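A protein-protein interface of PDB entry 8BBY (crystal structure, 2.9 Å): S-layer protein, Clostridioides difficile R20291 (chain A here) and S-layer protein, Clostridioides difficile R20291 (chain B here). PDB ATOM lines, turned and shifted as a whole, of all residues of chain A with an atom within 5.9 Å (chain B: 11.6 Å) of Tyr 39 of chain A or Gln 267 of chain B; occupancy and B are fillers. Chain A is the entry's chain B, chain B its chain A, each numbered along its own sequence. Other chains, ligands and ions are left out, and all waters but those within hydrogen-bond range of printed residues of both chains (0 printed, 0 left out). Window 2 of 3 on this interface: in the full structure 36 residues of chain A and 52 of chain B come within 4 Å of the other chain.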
ATOM      1  N   TYR A  28     -32.786  23.213 -33.386  1.00  0.00           N
ATOM      2  CA  TYR A  28     -31.382  23.464 -33.075  1.00  0.00           C
ATOM      3  C   TYR A  28     -31.009  24.917 -33.343  1.00  0.00           C
ATOM      4  O   TYR A  28     -30.242  25.516 -32.579  1.00  0.00           O
ATOM      5  CB  TYR A  28     -30.485  22.519 -33.874  1.00  0.00           C
ATOM      6  CG  TYR A  28     -29.071  22.433 -33.343  1.00  0.00           C
ATOM      7  CD1 TYR A  28     -28.087  23.309 -33.786  1.00  0.00           C
ATOM      8  CD2 TYR A  28     -28.722  21.482 -32.393  1.00  0.00           C
ATOM      9  CE1 TYR A  28     -26.793  23.236 -33.302  1.00  0.00           C
ATOM     10  CE2 TYR A  28     -27.431  21.401 -31.903  1.00  0.00           C
ATOM     11  CZ  TYR A  28     -26.471  22.280 -32.361  1.00  0.00           C
ATOM     12  OH  TYR A  28     -25.186  22.203 -31.875  1.00  0.00           O
ATOM     13  N   ASP A  31     -32.420  26.835 -30.450  1.00  0.00           N
ATOM     14  CA  ASP A  31     -31.570  26.688 -29.273  1.00  0.00           C
ATOM     15  C   ASP A  31     -30.272  27.470 -29.430  1.00  0.00           C
ATOM     16  O   ASP A  31     -29.794  28.092 -28.474  1.00  0.00           O
ATOM     17  CB  ASP A  31     -31.276  25.209 -29.019  1.00  0.00           C
ATOM     18  CG  ASP A  31     -32.406  24.505 -28.292  1.00  0.00           C
ATOM     19  OD1 ASP A  31     -33.555  24.991 -28.359  1.00  0.00           O
ATOM     20  OD2 ASP A  31     -32.145  23.462 -27.656  1.00  0.00           O
ATOM     21  N   LEU A  32     -29.685  27.443 -30.629  1.00  0.00           N
ATOM     22  CA  LEU A  32     -28.412  28.120 -30.854  1.00  0.00           C
ATOM     23  C   LEU A  32     -28.545  29.626 -30.662  1.00  0.00           C
ATOM     24  O   LEU A  32     -27.738  30.246 -29.961  1.00  0.00           O
ATOM     25  CB  LEU A  32     -27.888  27.801 -32.253  1.00  0.00           C
ATOM     26  CG  LEU A  32     -26.533  28.412 -32.613  1.00  0.00           C
ATOM     27  CD1 LEU A  32     -25.408  27.726 -31.849  1.00  0.00           C
ATOM     28  CD2 LEU A  32     -26.291  28.341 -34.114  1.00  0.00           C
ATOM     29  N   THR A  34     -30.632  31.288 -28.955  1.00  0.00           N
ATOM     30  CA  THR A  34     -30.941  31.677 -27.584  1.00  0.00           C
ATOM     31  C   THR A  34     -29.681  31.701 -26.728  1.00  0.00           C
ATOM     32  O   THR A  34     -29.386  32.704 -26.066  1.00  0.00           O
ATOM     33  CB  THR A  34     -31.979  30.727 -26.986  1.00  0.00           C
ATOM     34  OG1 THR A  34     -33.279  31.061 -27.489  1.00  0.00           O
ATOM     35  CG2 THR A  34     -31.989  30.831 -25.464  1.00  0.00           C
ATOM     36  N   TYR A  35     -28.919  30.605 -26.731  1.00  0.00           N
ATOM     37  CA  TYR A  35     -27.713  30.550 -25.917  1.00  0.00           C
ATOM     38  C   TYR A  35     -26.591  31.403 -26.491  1.00  0.00           C
ATOM     39  O   TYR A  35     -25.677  31.781 -25.749  1.00  0.00           O
ATOM     40  CB  TYR A  35     -27.248  29.102 -25.755  1.00  0.00           C
ATOM     41  CG  TYR A  35     -28.109  28.284 -24.815  1.00  0.00           C
ATOM     42  CD1 TYR A  35     -27.597  27.810 -23.620  1.00  0.00           C
ATOM     43  CD2 TYR A  35     -29.422  27.963 -25.134  1.00  0.00           C
ATOM     44  CE1 TYR A  35     -28.363  27.058 -22.755  1.00  0.00           C
ATOM     45  CE2 TYR A  35     -30.203  27.208 -24.273  1.00  0.00           C
ATOM     46  CZ  TYR A  35     -29.665  26.758 -23.085  1.00  0.00           C
ATOM     47  OH  TYR A  35     -30.429  26.006 -22.224  1.00  0.00           O
ATOM     48  N   ASN A  36     -26.634  31.711 -27.789  1.00  0.00           N
ATOM     49  CA  ASN A  36     -25.698  32.680 -28.347  1.00  0.00           C
ATOM     50  C   ASN A  36     -25.951  34.069 -27.779  1.00  0.00           C
ATOM     51  O   ASN A  36     -25.007  34.819 -27.507  1.00  0.00           O
ATOM     52  CB  ASN A  36     -25.802  32.698 -29.872  1.00  0.00           C
ATOM     53  CG  ASN A  36     -24.760  33.591 -30.518  1.00  0.00           C
ATOM     54  OD1 ASN A  36     -23.561  33.428 -30.295  1.00  0.00           O
ATOM     55  ND2 ASN A  36     -25.216  34.542 -31.326  1.00  0.00           N
ATOM     56  N   ASN A  37     -27.224  34.431 -27.600  1.00  0.00           N
ATOM     57  CA  ASN A  37     -27.556  35.734 -27.034  1.00  0.00           C
ATOM     58  C   ASN A  37     -27.156  35.819 -25.566  1.00  0.00           C
ATOM     59  O   ASN A  37     -26.690  36.867 -25.104  1.00  0.00           O
ATOM     60  CB  ASN A  37     -29.051  36.014 -27.199  1.00  0.00           C
ATOM     61  CG  ASN A  37     -29.445  36.298 -28.643  1.00  0.00           C
ATOM     62  OD1 ASN A  37     -30.155  37.264 -28.922  1.00  0.00           O
ATOM     63  ND2 ASN A  37     -28.990  35.456 -29.564  1.00  0.00           N
ATOM     64  N   GLY A  38     -27.340  34.733 -24.814  1.00  0.00           N
ATOM     65  CA  GLY A  38     -26.994  34.757 -23.402  1.00  0.00           C
ATOM     66  C   GLY A  38     -25.496  34.835 -23.163  1.00  0.00           C
ATOM     67  O   GLY A  38     -25.023  35.652 -22.368  1.00  0.00           O
ATOM     68  N   TYR A  39     -24.728  33.987 -23.854  1.00  0.00           N
ATOM     69  CA  TYR A  39     -23.287  33.949 -23.629  1.00  0.00           C
ATOM     70  C   TYR A  39     -22.608  35.230 -24.094  1.00  0.00           C
ATOM     71  O   TYR A  39     -21.570  35.616 -23.543  1.00  0.00           O
ATOM     72  CB  TYR A  39     -22.674  32.738 -24.333  1.00  0.00           C
ATOM     73  CG  TYR A  39     -22.247  31.643 -23.383  1.00  0.00           C
ATOM     74  CD1 TYR A  39     -21.298  31.884 -22.398  1.00  0.00           C
ATOM     75  CD2 TYR A  39     -22.799  30.371 -23.463  1.00  0.00           C
ATOM     76  CE1 TYR A  39     -20.905  30.888 -21.523  1.00  0.00           C
ATOM     77  CE2 TYR A  39     -22.414  29.369 -22.591  1.00  0.00           C
ATOM     78  CZ  TYR A  39     -21.467  29.633 -21.625  1.00  0.00           C
ATOM     79  OH  TYR A  39     -21.083  28.638 -20.755  1.00  0.00           O
ATOM     80  N   SER A  40     -23.170  35.898 -25.100  1.00  0.00           N
ATOM     81  CA  SER A  40     -22.605  37.149 -25.590  1.00  0.00           C
ATOM     82  C   SER A  40     -22.985  38.348 -24.734  1.00  0.00           C
ATOM     83  O   SER A  40     -22.404  39.424 -24.915  1.00  0.00           O
ATOM     84  CB  SER A  40     -23.047  37.394 -27.036  1.00  0.00           C
ATOM     85  OG  SER A  40     -22.368  36.535 -27.935  1.00  0.00           O
ATOM     86  N   ASN A  41     -23.932  38.194 -23.812  1.00  0.00           N
ATOM     87  CA  ASN A  41     -24.495  39.314 -23.069  1.00  0.00           C
ATOM     88  C   ASN A  41     -24.476  39.049 -21.569  1.00  0.00           C
ATOM     89  O   ASN A  41     -25.359  39.485 -20.827  1.00  0.00           O
ATOM     90  CB  ASN A  41     -25.914  39.612 -23.546  1.00  0.00           C
ATOM     91  CG  ASN A  41     -25.974  39.949 -25.029  1.00  0.00           C
ATOM     92  OD1 ASN A  41     -25.060  40.564 -25.580  1.00  0.00           O
ATOM     93  ND2 ASN A  41     -27.061  39.551 -25.682  1.00  0.00           N
ATOM     94  N   ALA A  42     -23.454  38.342 -21.094  1.00  0.00           N
ATOM     95  CA  ALA A  42     -23.246  38.162 -19.658  1.00  0.00           C
ATOM     96  C   ALA A  42     -21.750  37.951 -19.458  1.00  0.00           C
ATOM     97  O   ALA A  42     -21.233  36.881 -19.791  1.00  0.00           O
ATOM     98  CB  ALA A  42     -24.056  36.980 -19.126  1.00  0.00           C
ATOM     99  N   ILE A  43     -21.062  38.962 -18.916  1.00  0.00           N
ATOM    100  CA  ILE A  43     -19.602  38.997 -18.887  1.00  0.00           C
ATOM    101  C   ILE A  43     -19.108  39.302 -17.473  1.00  0.00           C
ATOM    102  O   ILE A  43     -19.744  40.051 -16.726  1.00  0.00           O
ATOM    103  CB  ILE A  43     -19.004  40.039 -19.877  1.00  0.00           C
ATOM    104  CG1 ILE A  43     -19.490  39.874 -21.329  1.00  0.00           C
ATOM    105  CG2 ILE A  43     -17.494  39.987 -19.854  1.00  0.00           C
ATOM    106  CD1 ILE A  43     -20.859  40.459 -21.669  1.00  0.00           C
ATOM    107  N   ILE B 256     -21.186  19.508 -38.502  1.00  0.00           N
ATOM    108  CA  ILE B 256     -21.775  18.937 -37.297  1.00  0.00           C
ATOM    109  C   ILE B 256     -23.121  18.329 -37.667  1.00  0.00           C
ATOM    110  O   ILE B 256     -23.988  19.012 -38.227  1.00  0.00           O
ATOM    111  CB  ILE B 256     -21.921  19.976 -36.172  1.00  0.00           C
ATOM    112  CG1 ILE B 256     -22.600  21.252 -36.676  1.00  0.00           C
ATOM    113  CG2 ILE B 256     -20.562  20.302 -35.570  1.00  0.00           C
ATOM    114  CD1 ILE B 256     -23.596  21.831 -35.694  1.00  0.00           C
ATOM    115  N   ILE B 258     -26.288  17.301 -36.141  1.00  0.00           N
ATOM    116  CA  ILE B 258     -26.988  17.514 -34.880  1.00  0.00           C
ATOM    117  C   ILE B 258     -27.795  16.294 -34.461  1.00  0.00           C
ATOM    118  O   ILE B 258     -28.190  16.190 -33.294  1.00  0.00           O
ATOM    119  CB  ILE B 258     -27.892  18.755 -34.980  1.00  0.00           C
ATOM    120  CG1 ILE B 258     -28.897  18.581 -36.115  1.00  0.00           C
ATOM    121  CG2 ILE B 258     -27.053  20.004 -35.205  1.00  0.00           C
ATOM    122  CD1 ILE B 258     -29.644  19.835 -36.442  1.00  0.00           C
ATOM    123  N   SER B 263     -21.673  15.369 -30.447  1.00  0.00           N
ATOM    124  CA  SER B 263     -21.651  16.658 -31.112  1.00  0.00           C
ATOM    125  C   SER B 263     -21.707  17.782 -30.086  1.00  0.00           C
ATOM    126  O   SER B 263     -22.186  17.611 -28.962  1.00  0.00           O
ATOM    127  CB  SER B 263     -22.824  16.783 -32.084  1.00  0.00           C
ATOM    128  OG  SER B 263     -22.695  15.891 -33.177  1.00  0.00           O
ATOM    129  N   LYS B 264     -21.211  18.948 -30.488  1.00  0.00           N
ATOM    130  CA  LYS B 264     -21.283  20.115 -29.621  1.00  0.00           C
ATOM    131  C   LYS B 264     -22.721  20.612 -29.537  1.00  0.00           C
ATOM    132  O   LYS B 264     -23.384  20.807 -30.560  1.00  0.00           O
ATOM    133  CB  LYS B 264     -20.365  21.219 -30.142  1.00  0.00           C
ATOM    134  CG  LYS B 264     -18.929  21.106 -29.656  1.00  0.00           C
ATOM    135  CD  LYS B 264     -18.035  22.147 -30.310  1.00  0.00           C
ATOM    136  CE  LYS B 264     -16.652  21.581 -30.594  1.00  0.00           C
ATOM    137  NZ  LYS B 264     -16.380  21.464 -32.055  1.00  0.00           N
ATOM    138  N   THR B 265     -23.203  20.810 -28.314  1.00  0.00           N
ATOM    139  CA  THR B 265     -24.545  21.331 -28.116  1.00  0.00           C
ATOM    140  C   THR B 265     -24.620  22.773 -28.613  1.00  0.00           C
ATOM    141  O   THR B 265     -23.602  23.444 -28.809  1.00  0.00           O
ATOM    142  CB  THR B 265     -24.936  21.256 -26.637  1.00  0.00           C
ATOM    143  OG1 THR B 265     -24.430  20.042 -26.070  1.00  0.00           O
ATOM    144  CG2 THR B 265     -26.452  21.274 -26.470  1.00  0.00           C
ATOM    145  N   ALA B 266     -25.850  23.244 -28.835  1.00  0.00           N
ATOM    146  CA  ALA B 266     -26.048  24.640 -29.208  1.00  0.00           C
ATOM    147  C   ALA B 266     -25.431  25.585 -28.183  1.00  0.00           C
ATOM    148  O   ALA B 266     -24.975  26.677 -28.542  1.00  0.00           O
ATOM    149  CB  ALA B 266     -27.537  24.932 -29.380  1.00  0.00           C
ATOM    150  N   GLN B 267     -25.408  25.185 -26.907  1.00  0.00           N
ATOM    151  CA  GLN B 267     -24.711  25.973 -25.895  1.00  0.00           C
ATOM    152  C   GLN B 267     -23.203  25.929 -26.100  1.00  0.00           C
ATOM    153  O   GLN B 267     -22.547  26.975 -26.180  1.00  0.00           O
ATOM    154  CB  GLN B 267     -25.063  25.472 -24.496  1.00  0.00           C
ATOM    155  CG  GLN B 267     -24.627  26.424 -23.393  1.00  0.00           C
ATOM    156  CD  GLN B 267     -24.033  25.714 -22.196  1.00  0.00           C
ATOM    157  OE1 GLN B 267     -23.763  24.514 -22.238  1.00  0.00           O
ATOM    158  NE2 GLN B 267     -23.838  26.455 -21.112  1.00  0.00           N
ATOM    159  N   ASP B 268     -22.633  24.723 -26.170  1.00  0.00           N
ATOM    160  CA  ASP B 268     -21.188  24.597 -26.318  1.00  0.00           C
ATOM    161  C   ASP B 268     -20.705  25.233 -27.613  1.00  0.00           C
ATOM    162  O   ASP B 268     -19.581  25.741 -27.675  1.00  0.00           O
ATOM    163  CB  ASP B 268     -20.780  23.125 -26.255  1.00  0.00           C
ATOM    164  CG  ASP B 268     -21.126  22.480 -24.924  1.00  0.00           C
ATOM    165  OD1 ASP B 268     -22.245  21.941 -24.795  1.00  0.00           O
ATOM    166  OD2 ASP B 268     -20.279  22.514 -24.007  1.00  0.00           O
ATOM    167  N   LEU B 269     -21.540  25.216 -28.654  1.00  0.00           N
ATOM    168  CA  LEU B 269     -21.212  25.949 -29.871  1.00  0.00           C
ATOM    169  C   LEU B 269     -21.260  27.454 -29.641  1.00  0.00           C
ATOM    170  O   LEU B 269     -20.461  28.196 -30.223  1.00  0.00           O
ATOM    171  CB  LEU B 269     -22.163  25.547 -30.997  1.00  0.00           C
ATOM    172  CG  LEU B 269     -21.585  25.571 -32.412  1.00  0.00           C
ATOM    173  CD1 LEU B 269     -20.486  24.531 -32.549  1.00  0.00           C
ATOM    174  CD2 LEU B 269     -22.677  25.336 -33.444  1.00  0.00           C
ATOM    175  N   ALA B 270     -22.183  27.920 -28.796  1.00  0.00           N
ATOM    176  CA  ALA B 270     -22.278  29.345 -28.496  1.00  0.00           C
ATOM    177  C   ALA B 270     -21.183  29.807 -27.543  1.00  0.00           C
ATOM    178  O   ALA B 270     -20.730  30.952 -27.640  1.00  0.00           O
ATOM    179  CB  ALA B 270     -23.652  29.666 -27.906  1.00  0.00           C
ATOM    180  N   LYS B 271     -20.756  28.946 -26.616  1.00  0.00           N
ATOM    181  CA  LYS B 271     -19.677  29.317 -25.707  1.00  0.00           C
ATOM    182  C   LYS B 271     -18.354  29.472 -26.447  1.00  0.00           C
ATOM    183  O   LYS B 271     -17.522  30.302 -26.063  1.00  0.00           O
ATOM    184  CB  LYS B 271     -19.553  28.277 -24.591  1.00  0.00           C
ATOM    185  CG  LYS B 271     -18.295  28.402 -23.744  1.00  0.00           C
ATOM    186  CD  LYS B 271     -18.479  27.776 -22.372  1.00  0.00           C
ATOM    187  CE  LYS B 271     -18.626  26.266 -22.463  1.00  0.00           C
ATOM    188  NZ  LYS B 271     -19.543  25.737 -21.415  1.00  0.00           N
ATOM    189  N   LYS B 272     -18.148  28.698 -27.511  1.00  0.00           N
ATOM    190  CA  LYS B 272     -16.908  28.745 -28.275  1.00  0.00           C
ATOM    191  C   LYS B 272     -16.952  29.770 -29.403  1.00  0.00           C
ATOM    192  O   LYS B 272     -15.963  30.471 -29.638  1.00  0.00           O
ATOM    193  CB  LYS B 272     -16.596  27.359 -28.846  1.00  0.00           C
ATOM    194  CG  LYS B 272     -15.228  27.237 -29.496  1.00  0.00           C
ATOM    195  CD  LYS B 272     -14.924  25.790 -29.847  1.00  0.00           C
ATOM    196  CE  LYS B 272     -13.618  25.664 -30.610  1.00  0.00           C
ATOM    197  NZ  LYS B 272     -13.374  24.263 -31.054  1.00  0.00           N
ATOM    198  N   TYR B 273     -18.080  29.878 -30.103  1.00  0.00           N
ATOM    199  CA  TYR B 273     -18.199  30.730 -31.276  1.00  0.00           C
ATOM    200  C   TYR B 273     -19.262  31.798 -31.060  1.00  0.00           C
ATOM    201  O   TYR B 273     -20.225  31.601 -30.313  1.00  0.00           O
ATOM    202  CB  TYR B 273     -18.550  29.912 -32.525  1.00  0.00           C
ATOM    203  CG  TYR B 273     -17.516  28.875 -32.893  1.00  0.00           C
ATOM    204  CD1 TYR B 273     -16.382  29.225 -33.612  1.00  0.00           C
ATOM    205  CD2 TYR B 273     -17.678  27.546 -32.528  1.00  0.00           C
ATOM    206  CE1 TYR B 273     -15.434  28.281 -33.952  1.00  0.00           C
ATOM    207  CE2 TYR B 273     -16.735  26.593 -32.866  1.00  0.00           C
ATOM    208  CZ  TYR B 273     -15.616  26.967 -33.578  1.00  0.00           C
ATOM    209  OH  TYR B 273     -14.674  26.023 -33.917  1.00  0.00           O
ATOM    210  N   VAL B 274     -19.079  32.931 -31.731  1.00  0.00           N
ATOM    211  CA  VAL B 274     -20.044  34.025 -31.722  1.00  0.00           C
ATOM    212  C   VAL B 274     -20.776  34.011 -33.058  1.00  0.00           C
ATOM    213  O   VAL B 274     -20.146  34.079 -34.119  1.00  0.00           O
ATOM    214  CB  VAL B 274     -19.359  35.378 -31.477  1.00  0.00           C
ATOM    215  CG1 VAL B 274     -20.400  36.477 -31.308  1.00  0.00           C
ATOM    216  CG2 VAL B 274     -18.454  35.302 -30.257  1.00  0.00           C
ATOM    217  N   PHE B 275     -22.101  33.924 -33.008  1.00  0.00           N
ATOM    218  CA  PHE B 275     -22.926  33.788 -34.198  1.00  0.00           C
ATOM    219  C   PHE B 275     -23.715  35.064 -34.458  1.00  0.00           C
ATOM    220  O   PHE B 275     -23.991  35.845 -33.542  1.00  0.00           O
ATOM    221  CB  PHE B 275     -23.896  32.608 -34.062  1.00  0.00           C
ATOM    222  CG  PHE B 275     -23.222  31.267 -34.058  1.00  0.00           C
ATOM    223  CD1 PHE B 275     -22.876  30.649 -35.247  1.00  0.00           C
ATOM    224  CD2 PHE B 275     -22.937  30.624 -32.865  1.00  0.00           C
ATOM    225  CE1 PHE B 275     -22.256  29.413 -35.247  1.00  0.00           C
ATOM    226  CE2 PHE B 275     -22.318  29.390 -32.857  1.00  0.00           C
ATOM    227  CZ  PHE B 275     -21.976  28.783 -34.051  1.00  0.00           C
ATOM    228  N   LYS B 277     -27.029  36.934 -35.013  1.00  0.00           N
ATOM    229  CA  LYS B 277     -28.390  36.660 -34.564  1.00  0.00           C
ATOM    230  C   LYS B 277     -29.399  36.809 -35.698  1.00  0.00           C
ATOM    231  O   LYS B 277     -30.362  36.038 -35.782  1.00  0.00           O
ATOM    232  CB  LYS B 277     -28.747  37.583 -33.400  1.00  0.00           C
ATOM    233  CG  LYS B 277     -27.732  37.561 -32.269  1.00  0.00           C
ATOM    234  CD  LYS B 277     -28.117  38.520 -31.157  1.00  0.00           C
ATOM    235  CE  LYS B 277     -27.054  38.556 -30.070  1.00  0.00           C
ATOM    236  NZ  LYS B 277     -27.451  39.435 -28.935  1.00  0.00           N
ATOM    237  N   LEU B 280     -29.510  33.762 -37.991  1.00  0.00           N
ATOM    238  CA  LEU B 280     -30.197  32.674 -37.306  1.00  0.00           C
ATOM    239  C   LEU B 280     -31.703  32.899 -37.265  1.00  0.00           C
ATOM    240  O   LEU B 280     -32.471  31.932 -37.204  1.00  0.00           O
ATOM    241  CB  LEU B 280     -29.645  32.514 -35.891  1.00  0.00           C
ATOM    242  CG  LEU B 280     -28.211  31.994 -35.785  1.00  0.00           C
ATOM    243  CD1 LEU B 280     -27.776  31.890 -34.332  1.00  0.00           C
ATOM    244  CD2 LEU B 280     -28.077  30.652 -36.485  1.00  0.00           C
ATOM    245  N   PRO B 311     -19.640  31.322 -38.250  1.00  0.00           N
ATOM    246  CA  PRO B 311     -19.512  32.204 -37.084  1.00  0.00           C
ATOM    247  C   PRO B 311     -18.807  33.497 -37.455  1.00  0.00           C
ATOM    248  O   PRO B 311     -18.402  33.684 -38.607  1.00  0.00           O
ATOM    249  CB  PRO B 311     -18.680  31.379 -36.092  1.00  0.00           C
ATOM    250  CG  PRO B 311     -18.540  30.020 -36.695  1.00  0.00           C
ATOM    251  CD  PRO B 311     -18.725  30.176 -38.168  1.00  0.00           C
ATOM    252  N   GLY B 313     -16.334  34.678 -35.105  1.00  0.00           N
ATOM    253  CA  GLY B 313     -15.090  34.635 -34.368  1.00  0.00           C
ATOM    254  C   GLY B 313     -15.192  33.697 -33.186  1.00  0.00           C
ATOM    255  O   GLY B 313     -16.235  33.097 -32.920  1.00  0.00           O
ATOM    256  N   LYS B 314     -14.073  33.585 -32.478  1.00  0.00           N
ATOM    257  CA  LYS B 314     -13.997  32.779 -31.270  1.00  0.00           C
ATOM    258  C   LYS B 314     -14.230  33.647 -30.040  1.00  0.00           C
ATOM    259  O   LYS B 314     -13.841  34.817 -29.999  1.00  0.00           O
ATOM    260  CB  LYS B 314     -12.641  32.078 -31.169  1.00  0.00           C
ATOM    261  CG  LYS B 314     -12.200  31.388 -32.451  1.00  0.00           C
ATOM    262  CD  LYS B 314     -10.717  31.596 -32.713  1.00  0.00           C
ATOM    263  CE  LYS B 314     -10.428  31.703 -34.202  1.00  0.00           C
ATOM    264  NZ  LYS B 314      -9.350  32.688 -34.493  1.00  0.00           N
ATOM    265  N   ARG B 315     -14.873  33.061 -29.034  1.00  0.00           N
ATOM    266  CA  ARG B 315     -15.200  33.789 -27.814  1.00  0.00           C
ATOM    267  C   ARG B 315     -13.972  33.857 -26.913  1.00  0.00           C
ATOM    268  O   ARG B 315     -13.398  32.823 -26.556  1.00  0.00           O
ATOM    269  CB  ARG B 315     -16.366  33.120 -27.089  1.00  0.00           C
ATOM    270  CG  ARG B 315     -17.259  34.092 -26.340  1.00  0.00           C
ATOM    271  CD  ARG B 315     -18.469  33.391 -25.739  1.00  0.00           C
ATOM    272  NE  ARG B 315     -19.523  33.155 -26.719  1.00  0.00           N
ATOM    273  CZ  ARG B 315     -20.302  34.099 -27.229  1.00  0.00           C
ATOM    274  NH1 ARG B 315     -20.173  35.367 -26.878  1.00  0.00           N
ATOM    275  NH2 ARG B 315     -21.237  33.761 -28.114  1.00  0.00           N
ATOM    276  N   VAL B 316     -13.577  35.071 -26.545  1.00  0.00           N
ATOM    277  CA  VAL B 316     -12.402  35.276 -25.706  1.00  0.00           C
ATOM    278  C   VAL B 316     -12.763  35.125 -24.233  1.00  0.00           C
ATOM    279  O   VAL B 316     -13.886  35.420 -23.825  1.00  0.00           O
ATOM    280  CB  VAL B 316     -11.762  36.651 -25.973  1.00  0.00           C
ATOM    281  CG1 VAL B 316     -12.797  37.757 -25.824  1.00  0.00           C
ATOM    282  CG2 VAL B 316     -10.588  36.880 -25.034  1.00  0.00           C
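Hydrophobic or aromatic side chains of chain A within 4 Å of the printed part of chain B: Tyr 28, Leu 32, Tyr 35 and Tyr 39.
Hydrophobic or aromatic side chains of chain B within 4 Å of the printed part of chain A: Ile 258, Ala 266, Leu 269, Ala 270, Val 274, Phe 275 and Leu 280.
Among the printed residues, no Asp or Glu carboxylate lies within 4 Å of a Lys or Arg side-chain nitrogen of the other chain.
Among the printed residues, merely in contact across the chains: Tyr 35 of chain A with Gln 267 of chain B (3.3 Å), Tyr 28 of chain A with Thr 265 of chain B (3.4 Å), Leu 32 of chain A with Ala 266 of chain B (3.5 Å), Tyr 39 of chain A with Gln 267 of chain B (3.5 Å), Tyr 28 of chain A with Ile 258 of chain B (3.6 Å), Asn 36 of chain A with Ala 270 of chain B (3.6 Å), Tyr 39 of chain A with Arg 315 of chain B (3.6 Å), Tyr 35 of chain A with Ala 270 of chain B (3.6 Å), Leu 32 of chain A with Phe 275 of chain B (3.7 Å), Asp 31 of chain A with Ala 266 of chain B (3.7 Å), Leu 32 of chain A with Leu 280 of chain B (3.8 Å), Asn 36 of chain A with Tyr 273 of chain B (3.8 Å), Asn 36 of chain A with Val 274 of chain B (3.8 Å), Ser 40 of chain A with Val 274 of chain B (3.9 Å) and Leu 32 of chain A with Leu 269 of chain B (3.96 Å).
Tyr 35 of chain A touches two residues of chain B.
No residue of chain B comes within 4 Å of Gly 38 of chain A.
Of chain B, only Gln 267, Lys 271 and Arg 315 come within 4 Å of Tyr 39 of chain A.
No residue of chain B comes within 4 Å of Ala 42 of chain A.
Of the printed residues of chain A, Gln 267 of chain B touches Tyr 35 (3.3 Å) and Tyr 39 (3.5 Å).
Of the printed residues of chain A, Leu 269 of chain B touches Leu 32.
Of the printed residues of chain A, Tyr 273 of chain B touches Asn 36.
Printed residues of chain A within 4 Å of Val 274 of chain B: Asn 36 (3.8 Å) and Ser 40 (3.9 Å).
Printed residues of chain A within 4 Å of Leu 280 of chain B: Leu 32.
Gly 313 of chain B touches none of the printed residues of chain A.
Lys 314 of chain B touches none of the printed residues of chain A.
The nearest residue of chain B that does not touch Tyr 39 of chain A is Ala 270 of chain B (4.2 Å).
The nearest residue of chain A that does not touch Gln 267 of chain B is Asp 31 of chain A (5.5 Å).
The nearest printed residue of chain A that does not touch Ala 270 of chain B is Tyr 39 of chain A (4.2 Å).
The backbone carbonyl oxygen of Tyr 273 of chain B lies within hydrogen-bond range of the guanidinium group of Arg 315 of chain B (3.2 Å).
The backbone carbonyl oxygen (O) of Asn 37 of chain A lies within hydrogen-bond range of the side-chain amide nitrogen (ND2) of Asn 41 of chain A (2.8 Å).
O of Asn 36 of chain A lies within hydrogen-bond range of OG of Ser 40 of chain A (3.2 Å).
OD1 of Asp 268 of chain B is in hydrogen-bond range of OG1 of Thr 265 of chain B.
O of Lys 272 of chain B lies within hydrogen-bond range of N of Arg 315 of chain B, 2.9 Å away.
The backbone carbonyl oxygen of Gly 313 of chain B lies within hydrogen-bond range of the backbone NH of Val 274 of chain B.
The backbone NH (N) of Ala 266 of chain B sits at hydrogen-bond distance from the side-chain hydroxyl (OH) of Tyr 28 of chain A (3.3 Å).
The side-chain hydroxyl (OH) of Tyr 28 of chain A is in hydrogen-bond range of the backbone carbonyl oxygen (O) of Lys 264 of chain B, at 2.6 Å.
O of Phe 275 of chain B lies within hydrogen-bond range of ND2 of Asn 36 of chain A, at 2.8 Å.
ND2 of Asn 41 of chain A sits close to NZ of Lys 277 of chain B (3.3 Å).
NH1 of Arg 315 of chain B lies within hydrogen-bond range of OG of Ser 40 of chain A, at 2.7 Å.
NH2 of Arg 315 of chain B sits at hydrogen-bond distance from OD1 of Asn 36 of chain A (3.2 Å).
NZ of Lys 271 of chain B lies close to OH of Tyr 39 of chain A (3.4 Å).
The side-chain amino group (NZ) of Lys 277 of chain B lies close to the side-chain amide oxygen (OD1) of Asn 37 of chain A, 3.5 Å away.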
